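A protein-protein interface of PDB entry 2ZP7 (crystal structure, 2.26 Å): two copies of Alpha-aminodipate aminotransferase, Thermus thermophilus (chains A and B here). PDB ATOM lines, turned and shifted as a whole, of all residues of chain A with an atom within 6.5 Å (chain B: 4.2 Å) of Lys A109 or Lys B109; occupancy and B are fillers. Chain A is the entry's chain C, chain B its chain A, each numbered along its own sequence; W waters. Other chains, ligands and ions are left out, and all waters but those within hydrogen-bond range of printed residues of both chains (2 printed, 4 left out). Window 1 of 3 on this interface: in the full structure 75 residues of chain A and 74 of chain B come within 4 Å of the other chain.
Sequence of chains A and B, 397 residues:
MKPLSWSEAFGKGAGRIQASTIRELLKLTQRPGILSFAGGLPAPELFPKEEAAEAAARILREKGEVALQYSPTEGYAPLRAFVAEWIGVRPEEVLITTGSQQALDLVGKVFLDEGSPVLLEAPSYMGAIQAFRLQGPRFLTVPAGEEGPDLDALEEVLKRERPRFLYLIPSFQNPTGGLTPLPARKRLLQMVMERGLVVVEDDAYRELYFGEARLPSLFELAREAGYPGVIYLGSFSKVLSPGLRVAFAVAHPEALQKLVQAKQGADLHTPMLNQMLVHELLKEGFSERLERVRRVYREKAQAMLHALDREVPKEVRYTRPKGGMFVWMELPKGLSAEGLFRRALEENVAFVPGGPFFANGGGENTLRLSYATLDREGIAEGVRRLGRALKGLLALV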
ATOM      1  N   GLY A  11     -26.013 -31.617  -0.806  1.00  0.00           N
ATOM      2  CA  GLY A  11     -26.936 -30.486  -0.941  1.00  0.00           C
ATOM      3  C   GLY A  11     -28.378 -30.937  -1.106  1.00  0.00           C
ATOM      4  O   GLY A  11     -28.688 -32.122  -0.978  1.00  0.00           O
ATOM      5  N   LYS A  12     -29.272 -29.998  -1.406  1.00  0.00           N
ATOM      6  CA  LYS A  12     -30.700 -30.337  -1.543  1.00  0.00           C
ATOM      7  C   LYS A  12     -30.987 -31.201  -2.762  1.00  0.00           C
ATOM      8  O   LYS A  12     -31.882 -32.043  -2.734  1.00  0.00           O
ATOM      9  CB  LYS A  12     -31.568 -29.084  -1.578  1.00  0.00           C
ATOM     10  CG  LYS A  12     -31.853 -28.494  -0.201  1.00  0.00           C
ATOM     11  CD  LYS A  12     -32.850 -27.328  -0.266  1.00  0.00           C
ATOM     12  CE  LYS A  12     -32.245 -26.075  -0.916  1.00  0.00           C
ATOM     13  NZ  LYS A  12     -33.118 -24.859  -0.760  1.00  0.00           N
ATOM     14  N   GLY A  13     -30.221 -31.007  -3.829  1.00  0.00           N
ATOM     15  CA  GLY A  13     -30.428 -31.760  -5.058  1.00  0.00           C
ATOM     16  C   GLY A  13     -30.338 -33.257  -4.828  1.00  0.00           C
ATOM     17  O   GLY A  13     -31.006 -34.042  -5.523  1.00  0.00           O
ATOM     18  N   ALA A  14     -29.520 -33.654  -3.845  1.00  0.00           N
ATOM     19  CA  ALA A  14     -29.332 -35.065  -3.525  1.00  0.00           C
ATOM     20  C   ALA A  14     -30.611 -35.678  -2.933  1.00  0.00           C
ATOM     21  O   ALA A  14     -30.914 -36.843  -3.164  1.00  0.00           O
ATOM     22  CB  ALA A  14     -28.166 -35.246  -2.584  1.00  0.00           C
ATOM     23  N   ILE A  17     -33.072 -36.433  -6.112  1.00  0.00           N
ATOM     24  CA  ILE A  17     -32.827 -37.457  -7.128  1.00  0.00           C
ATOM     25  C   ILE A  17     -33.028 -38.886  -6.591  1.00  0.00           C
ATOM     26  O   ILE A  17     -32.868 -39.859  -7.335  1.00  0.00           O
ATOM     27  CB  ILE A  17     -31.442 -37.283  -7.814  1.00  0.00           C
ATOM     28  CG1 ILE A  17     -30.356 -36.962  -6.795  1.00  0.00           C
ATOM     29  CG2 ILE A  17     -31.493 -36.214  -8.881  1.00  0.00           C
ATOM     30  CD1 ILE A  17     -29.335 -38.037  -6.685  1.00  0.00           C
ATOM     31  N   LEU A 104     -34.660 -32.763 -21.680  1.00  0.00           N
ATOM     32  CA  LEU A 104     -35.456 -32.624 -20.443  1.00  0.00           C
ATOM     33  C   LEU A 104     -34.673 -32.061 -19.255  1.00  0.00           C
ATOM     34  O   LEU A 104     -35.174 -31.218 -18.507  1.00  0.00           O
ATOM     35  CB  LEU A 104     -36.062 -33.978 -20.027  1.00  0.00           C
ATOM     36  CG  LEU A 104     -37.035 -34.584 -21.021  1.00  0.00           C
ATOM     37  CD1 LEU A 104     -37.302 -36.063 -20.656  1.00  0.00           C
ATOM     38  CD2 LEU A 104     -38.335 -33.746 -21.074  1.00  0.00           C
ATOM     39  N   ASP A 105     -33.466 -32.577 -19.048  1.00  0.00           N
ATOM     40  CA  ASP A 105     -32.572 -32.085 -17.992  1.00  0.00           C
ATOM     41  C   ASP A 105     -32.376 -30.602 -18.232  1.00  0.00           C
ATOM     42  O   ASP A 105     -32.496 -29.806 -17.319  1.00  0.00           O
ATOM     43  CB  ASP A 105     -31.222 -32.842 -18.078  1.00  0.00           C
ATOM     44  CG  ASP A 105     -30.170 -32.371 -17.051  1.00  0.00           C
ATOM     45  OD1 ASP A 105     -30.482 -32.233 -15.869  1.00  0.00           O
ATOM     46  OD2 ASP A 105     -29.006 -32.150 -17.444  1.00  0.00           O
ATOM     47  N   LEU A 106     -32.100 -30.242 -19.485  1.00  0.00           N
ATOM     48  CA  LEU A 106     -31.722 -28.878 -19.855  1.00  0.00           C
ATOM     49  C   LEU A 106     -32.902 -27.931 -19.753  1.00  0.00           C
ATOM     50  O   LEU A 106     -32.767 -26.804 -19.287  1.00  0.00           O
ATOM     51  CB  LEU A 106     -31.160 -28.858 -21.282  1.00  0.00           C
ATOM     52  CG  LEU A 106     -29.876 -29.650 -21.593  1.00  0.00           C
ATOM     53  CD1 LEU A 106     -29.525 -29.534 -23.092  1.00  0.00           C
ATOM     54  CD2 LEU A 106     -28.711 -29.206 -20.712  1.00  0.00           C
ATOM     55  N   VAL A 107     -34.063 -28.396 -20.203  1.00  0.00           N
ATOM     56  CA  VAL A 107     -35.311 -27.695 -20.028  1.00  0.00           C
ATOM     57  C   VAL A 107     -35.539 -27.413 -18.540  1.00  0.00           C
ATOM     58  O   VAL A 107     -35.929 -26.304 -18.170  1.00  0.00           O
ATOM     59  CB  VAL A 107     -36.476 -28.495 -20.731  1.00  0.00           C
ATOM     60  CG1 VAL A 107     -37.842 -28.252 -20.077  1.00  0.00           C
ATOM     61  CG2 VAL A 107     -36.485 -28.210 -22.300  1.00  0.00           C
ATOM     62  N   GLY A 108     -35.253 -28.386 -17.676  1.00  0.00           N
ATOM     63  CA  GLY A 108     -35.468 -28.189 -16.234  1.00  0.00           C
ATOM     64  C   GLY A 108     -34.588 -27.083 -15.647  1.00  0.00           C
ATOM     65  O   GLY A 108     -35.038 -26.245 -14.851  1.00  0.00           O
ATOM     66  N   LYS A 109     -33.316 -27.090 -16.037  1.00  0.00           N
ATOM     67  CA  LYS A 109     -32.357 -26.111 -15.549  1.00  0.00           C
ATOM     68  C   LYS A 109     -32.718 -24.688 -15.979  1.00  0.00           C
ATOM     69  O   LYS A 109     -32.583 -23.753 -15.182  1.00  0.00           O
ATOM     70  CB  LYS A 109     -30.959 -26.450 -16.062  1.00  0.00           C
ATOM     71  CG  LYS A 109     -30.402 -27.799 -15.586  1.00  0.00           C
ATOM     72  CD  LYS A 109     -29.276 -28.226 -16.518  1.00  0.00           C
ATOM     73  CE  LYS A 109     -28.447 -29.319 -15.868  1.00  0.00           C
ATOM     74  NZ  LYS A 109     -27.325 -29.689 -16.731  1.00  0.00           N
ATOM     75  N   VAL A 110     -33.145 -24.506 -17.232  1.00  0.00           N
ATOM     76  CA  VAL A 110     -33.410 -23.148 -17.683  1.00  0.00           C
ATOM     77  C   VAL A 110     -34.773 -22.596 -17.265  1.00  0.00           C
ATOM     78  O   VAL A 110     -34.939 -21.381 -17.191  1.00  0.00           O
ATOM     79  CB  VAL A 110     -33.060 -22.845 -19.196  1.00  0.00           C
ATOM     80  CG1 VAL A 110     -32.001 -23.766 -19.759  1.00  0.00           C
ATOM     81  CG2 VAL A 110     -34.275 -22.758 -20.069  1.00  0.00           C
ATOM     82  N   PHE A 111     -35.726 -23.477 -16.955  1.00  0.00           N
ATOM     83  CA  PHE A 111     -37.101 -23.031 -16.702  1.00  0.00           C
ATOM     84  C   PHE A 111     -37.579 -23.102 -15.254  1.00  0.00           C
ATOM     85  O   PHE A 111     -38.493 -22.377 -14.870  1.00  0.00           O
ATOM     86  CB  PHE A 111     -38.091 -23.749 -17.624  1.00  0.00           C
ATOM     87  CG  PHE A 111     -38.068 -23.247 -19.042  1.00  0.00           C
ATOM     88  CD1 PHE A 111     -38.662 -22.026 -19.370  1.00  0.00           C
ATOM     89  CD2 PHE A 111     -37.440 -23.988 -20.048  1.00  0.00           C
ATOM     90  CE1 PHE A 111     -38.626 -21.551 -20.675  1.00  0.00           C
ATOM     91  CE2 PHE A 111     -37.398 -23.532 -21.345  1.00  0.00           C
ATOM     92  CZ  PHE A 111     -38.000 -22.306 -21.672  1.00  0.00           C
ATOM     93  N   LEU A 112     -36.962 -23.968 -14.468  1.00  0.00           N
ATOM     94  CA  LEU A 112     -37.498 -24.328 -13.173  1.00  0.00           C
ATOM     95  C   LEU A 112     -36.602 -23.834 -12.043  1.00  0.00           C
ATOM     96  O   LEU A 112     -35.374 -23.787 -12.186  1.00  0.00           O
ATOM     97  CB  LEU A 112     -37.693 -25.857 -13.062  1.00  0.00           C
ATOM     98  CG  LEU A 112     -38.687 -26.538 -13.992  1.00  0.00           C
ATOM     99  CD1 LEU A 112     -38.790 -28.063 -13.721  1.00  0.00           C
ATOM    100  CD2 LEU A 112     -40.047 -25.874 -13.885  1.00  0.00           C
ATOM    101  N   ASP A 113     -37.253 -23.463 -10.940  1.00  0.00           N
ATOM    102  CA  ASP A 113     -36.613 -23.087  -9.675  1.00  0.00           C
ATOM    103  C   ASP A 113     -37.315 -23.844  -8.576  1.00  0.00           C
ATOM    104  O   ASP A 113     -38.332 -24.486  -8.814  1.00  0.00           O
ATOM    105  CB  ASP A 113     -36.779 -21.591  -9.394  1.00  0.00           C
ATOM    106  CG  ASP A 113     -36.143 -20.736 -10.444  1.00  0.00           C
ATOM    107  OD1 ASP A 113     -34.967 -21.002 -10.767  1.00  0.00           O
ATOM    108  OD2 ASP A 113     -36.800 -19.797 -10.938  1.00  0.00           O
ATOM    109  N   ALA A 131     -35.974 -35.710 -14.300  1.00  0.00           N
ATOM    110  CA  ALA A 131     -35.199 -34.553 -14.728  1.00  0.00           C
ATOM    111  C   ALA A 131     -35.689 -33.289 -14.045  1.00  0.00           C
ATOM    112  O   ALA A 131     -34.870 -32.498 -13.578  1.00  0.00           O
ATOM    113  CB  ALA A 131     -35.258 -34.385 -16.217  1.00  0.00           C
ATOM    114  N   LEU A 134     -35.363 -32.641  -9.936  1.00  0.00           N
ATOM    115  CA  LEU A 134     -34.068 -32.181  -9.562  1.00  0.00           C
ATOM    116  C   LEU A 134     -34.106 -30.723  -9.131  1.00  0.00           C
ATOM    117  O   LEU A 134     -33.292 -30.315  -8.319  1.00  0.00           O
ATOM    118  CB  LEU A 134     -33.164 -32.310 -10.789  1.00  0.00           C
ATOM    119  CG  LEU A 134     -31.673 -32.582 -10.721  1.00  0.00           C
ATOM    120  CD1 LEU A 134     -31.054 -32.053 -11.992  1.00  0.00           C
ATOM    121  CD2 LEU A 134     -31.024 -31.965  -9.504  1.00  0.00           C
ATOM    122  N   GLN A 135     -35.046 -29.943  -9.687  1.00  0.00           N
ATOM    123  CA  GLN A 135     -35.084 -28.500  -9.456  1.00  0.00           C
ATOM    124  C   GLN A 135     -35.978 -28.104  -8.258  1.00  0.00           C
ATOM    125  O   GLN A 135     -36.047 -26.922  -7.878  1.00  0.00           O
ATOM    126  CB  GLN A 135     -35.486 -27.729 -10.735  1.00  0.00           C
ATOM    127  CG  GLN A 135     -34.719 -28.083 -12.045  1.00  0.00           C
ATOM    128  CD  GLN A 135     -33.184 -27.914 -11.968  1.00  0.00           C
ATOM    129  OE1 GLN A 135     -32.439 -28.601 -12.682  1.00  0.00           O
ATOM    130  NE2 GLN A 135     -32.714 -27.018 -11.089  1.00  0.00           N
ATOM    131  N   ALA A 262     -26.788 -24.145 -21.541  1.00  0.00           N
ATOM    132  CA  ALA A 262     -26.853 -25.120 -20.478  1.00  0.00           C
ATOM    133  C   ALA A 262     -26.098 -26.411 -20.870  1.00  0.00           C
ATOM    134  O   ALA A 262     -25.370 -26.976 -20.056  1.00  0.00           O
ATOM    135  CB  ALA A 262     -28.317 -25.405 -20.100  1.00  0.00           C
ATOM    136  N   LYS A 263     -26.278 -26.864 -22.111  1.00  0.00           N
ATOM    137  CA  LYS A 263     -25.556 -28.025 -22.648  1.00  0.00           C
ATOM    138  C   LYS A 263     -24.032 -27.913 -22.543  1.00  0.00           C
ATOM    139  O   LYS A 263     -23.365 -28.903 -22.224  1.00  0.00           O
ATOM    140  CB  LYS A 263     -25.952 -28.310 -24.110  1.00  0.00           C
ATOM    141  CG  LYS A 263     -25.452 -29.678 -24.634  1.00  0.00           C
ATOM    142  CD  LYS A 263     -25.766 -29.872 -26.099  1.00  0.00           C
ATOM    143  CE  LYS A 263     -24.916 -30.954 -26.712  1.00  0.00           C
ATOM    144  NZ  LYS A 263     -25.097 -32.265 -26.062  1.00  0.00           N
ATOM    145  N   GLY A 265     -22.267 -26.781 -20.239  1.00  0.00           N
ATOM    146  CA  GLY A 265     -21.889 -27.200 -18.894  1.00  0.00           C
ATOM    147  C   GLY A 265     -22.307 -28.612 -18.527  1.00  0.00           C
ATOM    148  O   GLY A 265     -21.842 -29.140 -17.519  1.00  0.00           O
ATOM    149  N   ALA A 266     -23.160 -29.225 -19.349  1.00  0.00           N
ATOM    150  CA  ALA A 266     -23.662 -30.585 -19.111  1.00  0.00           C
ATOM    151  C   ALA A 266     -22.719 -31.667 -19.645  1.00  0.00           C
ATOM    152  O   ALA A 266     -22.339 -32.541 -18.900  1.00  0.00           O
ATOM    153  CB  ALA A 266     -25.068 -30.751 -19.685  1.00  0.00           C
ATOM    154  N   GLY B  13     -31.838 -20.389 -13.244  1.00  0.00           N
ATOM    155  CA  GLY B  13     -30.771 -21.084 -13.964  1.00  0.00           C
ATOM    156  C   GLY B  13     -30.349 -20.451 -15.276  1.00  0.00           C
ATOM    157  O   GLY B  13     -29.162 -20.480 -15.632  1.00  0.00           O
ATOM    158  N   ALA B  14     -31.314 -19.857 -15.974  1.00  0.00           N
ATOM    159  CA  ALA B  14     -31.072 -19.179 -17.245  1.00  0.00           C
ATOM    160  C   ALA B  14     -30.144 -17.971 -17.088  1.00  0.00           C
ATOM    161  O   ALA B  14     -29.401 -17.624 -18.006  1.00  0.00           O
ATOM    162  CB  ALA B  14     -32.389 -18.767 -17.894  1.00  0.00           C
ATOM    163  N   ASP B 105     -20.851 -31.524 -13.747  1.00  0.00           N
ATOM    164  CA  ASP B 105     -22.288 -31.227 -13.635  1.00  0.00           C
ATOM    165  C   ASP B 105     -22.944 -32.032 -12.526  1.00  0.00           C
ATOM    166  O   ASP B 105     -23.702 -31.480 -11.728  1.00  0.00           O
ATOM    167  CB  ASP B 105     -22.988 -31.471 -14.990  1.00  0.00           C
ATOM    168  CG  ASP B 105     -24.454 -31.049 -14.999  1.00  0.00           C
ATOM    169  OD1 ASP B 105     -24.778 -29.890 -14.673  1.00  0.00           O
ATOM    170  OD2 ASP B 105     -25.295 -31.898 -15.350  1.00  0.00           O
ATOM    171  N   LEU B 106     -22.657 -33.335 -12.471  1.00  0.00           N
ATOM    172  CA  LEU B 106     -23.285 -34.201 -11.476  1.00  0.00           C
ATOM    173  C   LEU B 106     -22.874 -33.851 -10.068  1.00  0.00           C
ATOM    174  O   LEU B 106     -23.722 -33.808  -9.180  1.00  0.00           O
ATOM    175  CB  LEU B 106     -23.031 -35.704 -11.750  1.00  0.00           C
ATOM    176  CG  LEU B 106     -23.364 -36.200 -13.163  1.00  0.00           C
ATOM    177  CD1 LEU B 106     -22.905 -37.695 -13.334  1.00  0.00           C
ATOM    178  CD2 LEU B 106     -24.858 -35.968 -13.530  1.00  0.00           C
ATOM    179  N   VAL B 107     -21.589 -33.575  -9.871  1.00  0.00           N
ATOM    180  CA  VAL B 107     -21.083 -33.087  -8.586  1.00  0.00           C
ATOM    181  C   VAL B 107     -21.733 -31.771  -8.165  1.00  0.00           C
ATOM    182  O   VAL B 107     -22.083 -31.593  -7.001  1.00  0.00           O
ATOM    183  CB  VAL B 107     -19.532 -32.997  -8.588  1.00  0.00           C
ATOM    184  CG1 VAL B 107     -19.038 -32.070  -7.532  1.00  0.00           C
ATOM    185  CG2 VAL B 107     -18.898 -34.413  -8.409  1.00  0.00           C
ATOM    186  N   GLY B 108     -21.923 -30.858  -9.108  1.00  0.00           N
ATOM    187  CA  GLY B 108     -22.666 -29.622  -8.826  1.00  0.00           C
ATOM    188  C   GLY B 108     -24.077 -29.925  -8.347  1.00  0.00           C
ATOM    189  O   GLY B 108     -24.530 -29.381  -7.341  1.00  0.00           O
ATOM    190  N   LYS B 109     -24.768 -30.814  -9.052  1.00  0.00           N
ATOM    191  CA  LYS B 109     -26.121 -31.203  -8.674  1.00  0.00           C
ATOM    192  C   LYS B 109     -26.270 -31.830  -7.299  1.00  0.00           C
ATOM    193  O   LYS B 109     -27.171 -31.468  -6.562  1.00  0.00           O
ATOM    194  CB  LYS B 109     -26.709 -32.127  -9.716  1.00  0.00           C
ATOM    195  CG  LYS B 109     -26.961 -31.431 -11.057  1.00  0.00           C
ATOM    196  CD  LYS B 109     -27.277 -32.497 -12.103  1.00  0.00           C
ATOM    197  CE  LYS B 109     -27.766 -31.906 -13.398  1.00  0.00           C
ATOM    198  NZ  LYS B 109     -27.987 -32.979 -14.411  1.00  0.00           N
ATOM    199  N   VAL B 110     -25.374 -32.743  -6.941  1.00  0.00           N
ATOM    200  CA  VAL B 110     -25.474 -33.480  -5.685  1.00  0.00           C
ATOM    201  C   VAL B 110     -25.024 -32.653  -4.481  1.00  0.00           C
ATOM    202  O   VAL B 110     -25.562 -32.827  -3.398  1.00  0.00           O
ATOM    203  CB  VAL B 110     -24.756 -34.899  -5.766  1.00  0.00           C
ATOM    204  CG1 VAL B 110     -23.430 -34.777  -6.390  1.00  0.00           C
ATOM    205  CG2 VAL B 110     -24.614 -35.558  -4.387  1.00  0.00           C
ATOM    206  N   PHE B 111     -24.092 -31.720  -4.681  1.00  0.00           N
ATOM    207  CA  PHE B 111     -23.451 -31.034  -3.557  1.00  0.00           C
ATOM    208  C   PHE B 111     -23.789 -29.566  -3.346  1.00  0.00           C
ATOM    209  O   PHE B 111     -23.696 -29.088  -2.221  1.00  0.00           O
ATOM    210  CB  PHE B 111     -21.927 -31.204  -3.629  1.00  0.00           C
ATOM    211  CG  PHE B 111     -21.474 -32.612  -3.390  1.00  0.00           C
ATOM    212  CD1 PHE B 111     -21.426 -33.122  -2.104  1.00  0.00           C
ATOM    213  CD2 PHE B 111     -21.083 -33.412  -4.444  1.00  0.00           C
ATOM    214  CE1 PHE B 111     -21.024 -34.456  -1.867  1.00  0.00           C
ATOM    215  CE2 PHE B 111     -20.674 -34.738  -4.236  1.00  0.00           C
ATOM    216  CZ  PHE B 111     -20.647 -35.256  -2.928  1.00  0.00           C
ATOM    217  N   LEU B 134     -24.115 -22.884 -12.426  1.00  0.00           N
ATOM    218  CA  LEU B 134     -25.502 -23.240 -12.705  1.00  0.00           C
ATOM    219  C   LEU B 134     -26.315 -23.314 -11.400  1.00  0.00           C
ATOM    220  O   LEU B 134     -27.486 -22.943 -11.385  1.00  0.00           O
ATOM    221  CB  LEU B 134     -25.543 -24.601 -13.391  1.00  0.00           C
ATOM    222  CG  LEU B 134     -26.582 -25.039 -14.438  1.00  0.00           C
ATOM    223  CD1 LEU B 134     -26.834 -26.526 -14.251  1.00  0.00           C
ATOM    224  CD2 LEU B 134     -27.912 -24.272 -14.421  1.00  0.00           C
ATOM    225  N   GLN B 135     -25.683 -23.797 -10.325  1.00  0.00           N
ATOM    226  CA  GLN B 135     -26.371 -24.000  -9.039  1.00  0.00           C
ATOM    227  C   GLN B 135     -26.469 -22.742  -8.161  1.00  0.00           C
ATOM    228  O   GLN B 135     -27.060 -22.781  -7.082  1.00  0.00           O
ATOM    229  CB  GLN B 135     -25.718 -25.139  -8.232  1.00  0.00           C
ATOM    230  CG  GLN B 135     -25.384 -26.419  -9.008  1.00  0.00           C
ATOM    231  CD  GLN B 135     -26.602 -27.075  -9.609  1.00  0.00           C
ATOM    232  OE1 GLN B 135     -26.545 -27.701 -10.685  1.00  0.00           O
ATOM    233  NE2 GLN B 135     -27.722 -26.931  -8.934  1.00  0.00           N
ATOM    234  N   ALA B 266     -29.728 -37.233 -16.095  1.00  0.00           N
ATOM    235  CA  ALA B 266     -28.987 -36.390 -17.012  1.00  0.00           C
ATOM    236  C   ALA B 266     -29.053 -36.874 -18.461  1.00  0.00           C
ATOM    237  O   ALA B 266     -29.359 -36.080 -19.361  1.00  0.00           O
ATOM    238  CB  ALA B 266     -27.524 -36.219 -16.547  1.00  0.00           C
HETATM  239  O   HOH W   1     -27.670 -33.739 -19.409  1.00  0.00           O
HETATM  240  O   HOH W   2     -27.547 -30.084  -4.272  1.00  0.00           O
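The backbone carbonyl oxygen of Val B110 sits at hydrogen-bond distance from the backbone NH of Gly A11 (2.9 Å). The side-chain amino group (NZ) of Lys A109 is in salt-bridge range of the side-chain carboxylate (OD1) of Asp B105. The side-chain carboxylate of Asp A105 is in salt-bridge range of the side-chain amino group of Lys B109, 3.0 Å away.
Water W2 lies within hydrogen-bond range of O of Lys B109, N of Gly A13, N of Lys A12 and O of Val B110. Water W1 bridges the side-chain carboxylate of Asp A105 (2.9 Å) and the backbone carbonyl oxygen of Ala B266 (2.9 Å).
Lys A109 touches just these residues of chain B: Gly B13, Asp B105, Lys B109 and Leu B134. Printed residues of chain A within 4 Å of Lys B109: Gly A13 (3.6 Å), Asp A105 (3.0 Å), Lys A109 (3.6 Å) and Leu A134 (3.6 Å). Printed residues of chain B within 4 Å of Ala A14: Val B110. Of the printed residues of chain A, Ala B266 touches Asp A105 (3.9 Å). Leu A106 touches none of the printed residues of chain B. Leu A104 touches none of the printed residues of chain B. The nearest printed residue of chain A that does not touch Gly B13 is Asp A113 (4.04 Å).
NZ of Lys A109 is in salt-bridge range of OD2 of Asp A105, 3.1 Å away. The side-chain amino group (NZ) of Lys B109 is in salt-bridge range of the side-chain carboxylate (OD2) of Asp B105 (3.0 Å).
Among the printed residues, pairs that only touch across the chains: Gly A11 with Phe B111 (3.7 Å), Gly A13 with Lys B109 (3.6 Å), Ala A14 with Val B110 (3.6 Å), Asp A105 with Ala B266 (3.9 Å), Lys A109 with Gly B13 (3.4 Å), Lys A109 with Lys B109 (3.6 Å), Lys A109 with Leu B134 (3.6 Å), Val A110 with Ala B14 (3.7 Å), Leu A134 with Lys B109 (3.6 Å) and Gly A265 with Asp B105 (3.6 Å).
Gly A13 touches Lys B109, and with the chains exchanged Lys A109 touches Gly B13. Ala A14 touches Val B110, and with the chains exchanged Val A110 touches Ala B14. Asp A105 touches Lys B109, and with the chains exchanged Lys A109 touches Asp B105. Lys A109 touches Leu B134, and with the chains exchanged Leu A134 touches Lys B109. Of the 13 pairs that touch across the chains among the printed residues, 9 have their exchanged pair printed and touching as well.
Along chain A the printed residues that touch a printed residue of chain B span positions 11 to 265. Hydrophobic or aromatic side chains of chain B within 4 Å of the printed part of chain A: Ala B14, Val B110 and Leu B134. Among the printed residues, 13 pairs touch across the chains. Among the printed residues, Asp or Glu carboxylates within 4 Å of a Lys or Arg side-chain nitrogen of the other chain: Asp A105 with Lys B109 (3.0 Å) and Lys A109 with Asp B105 (3.3 Å).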
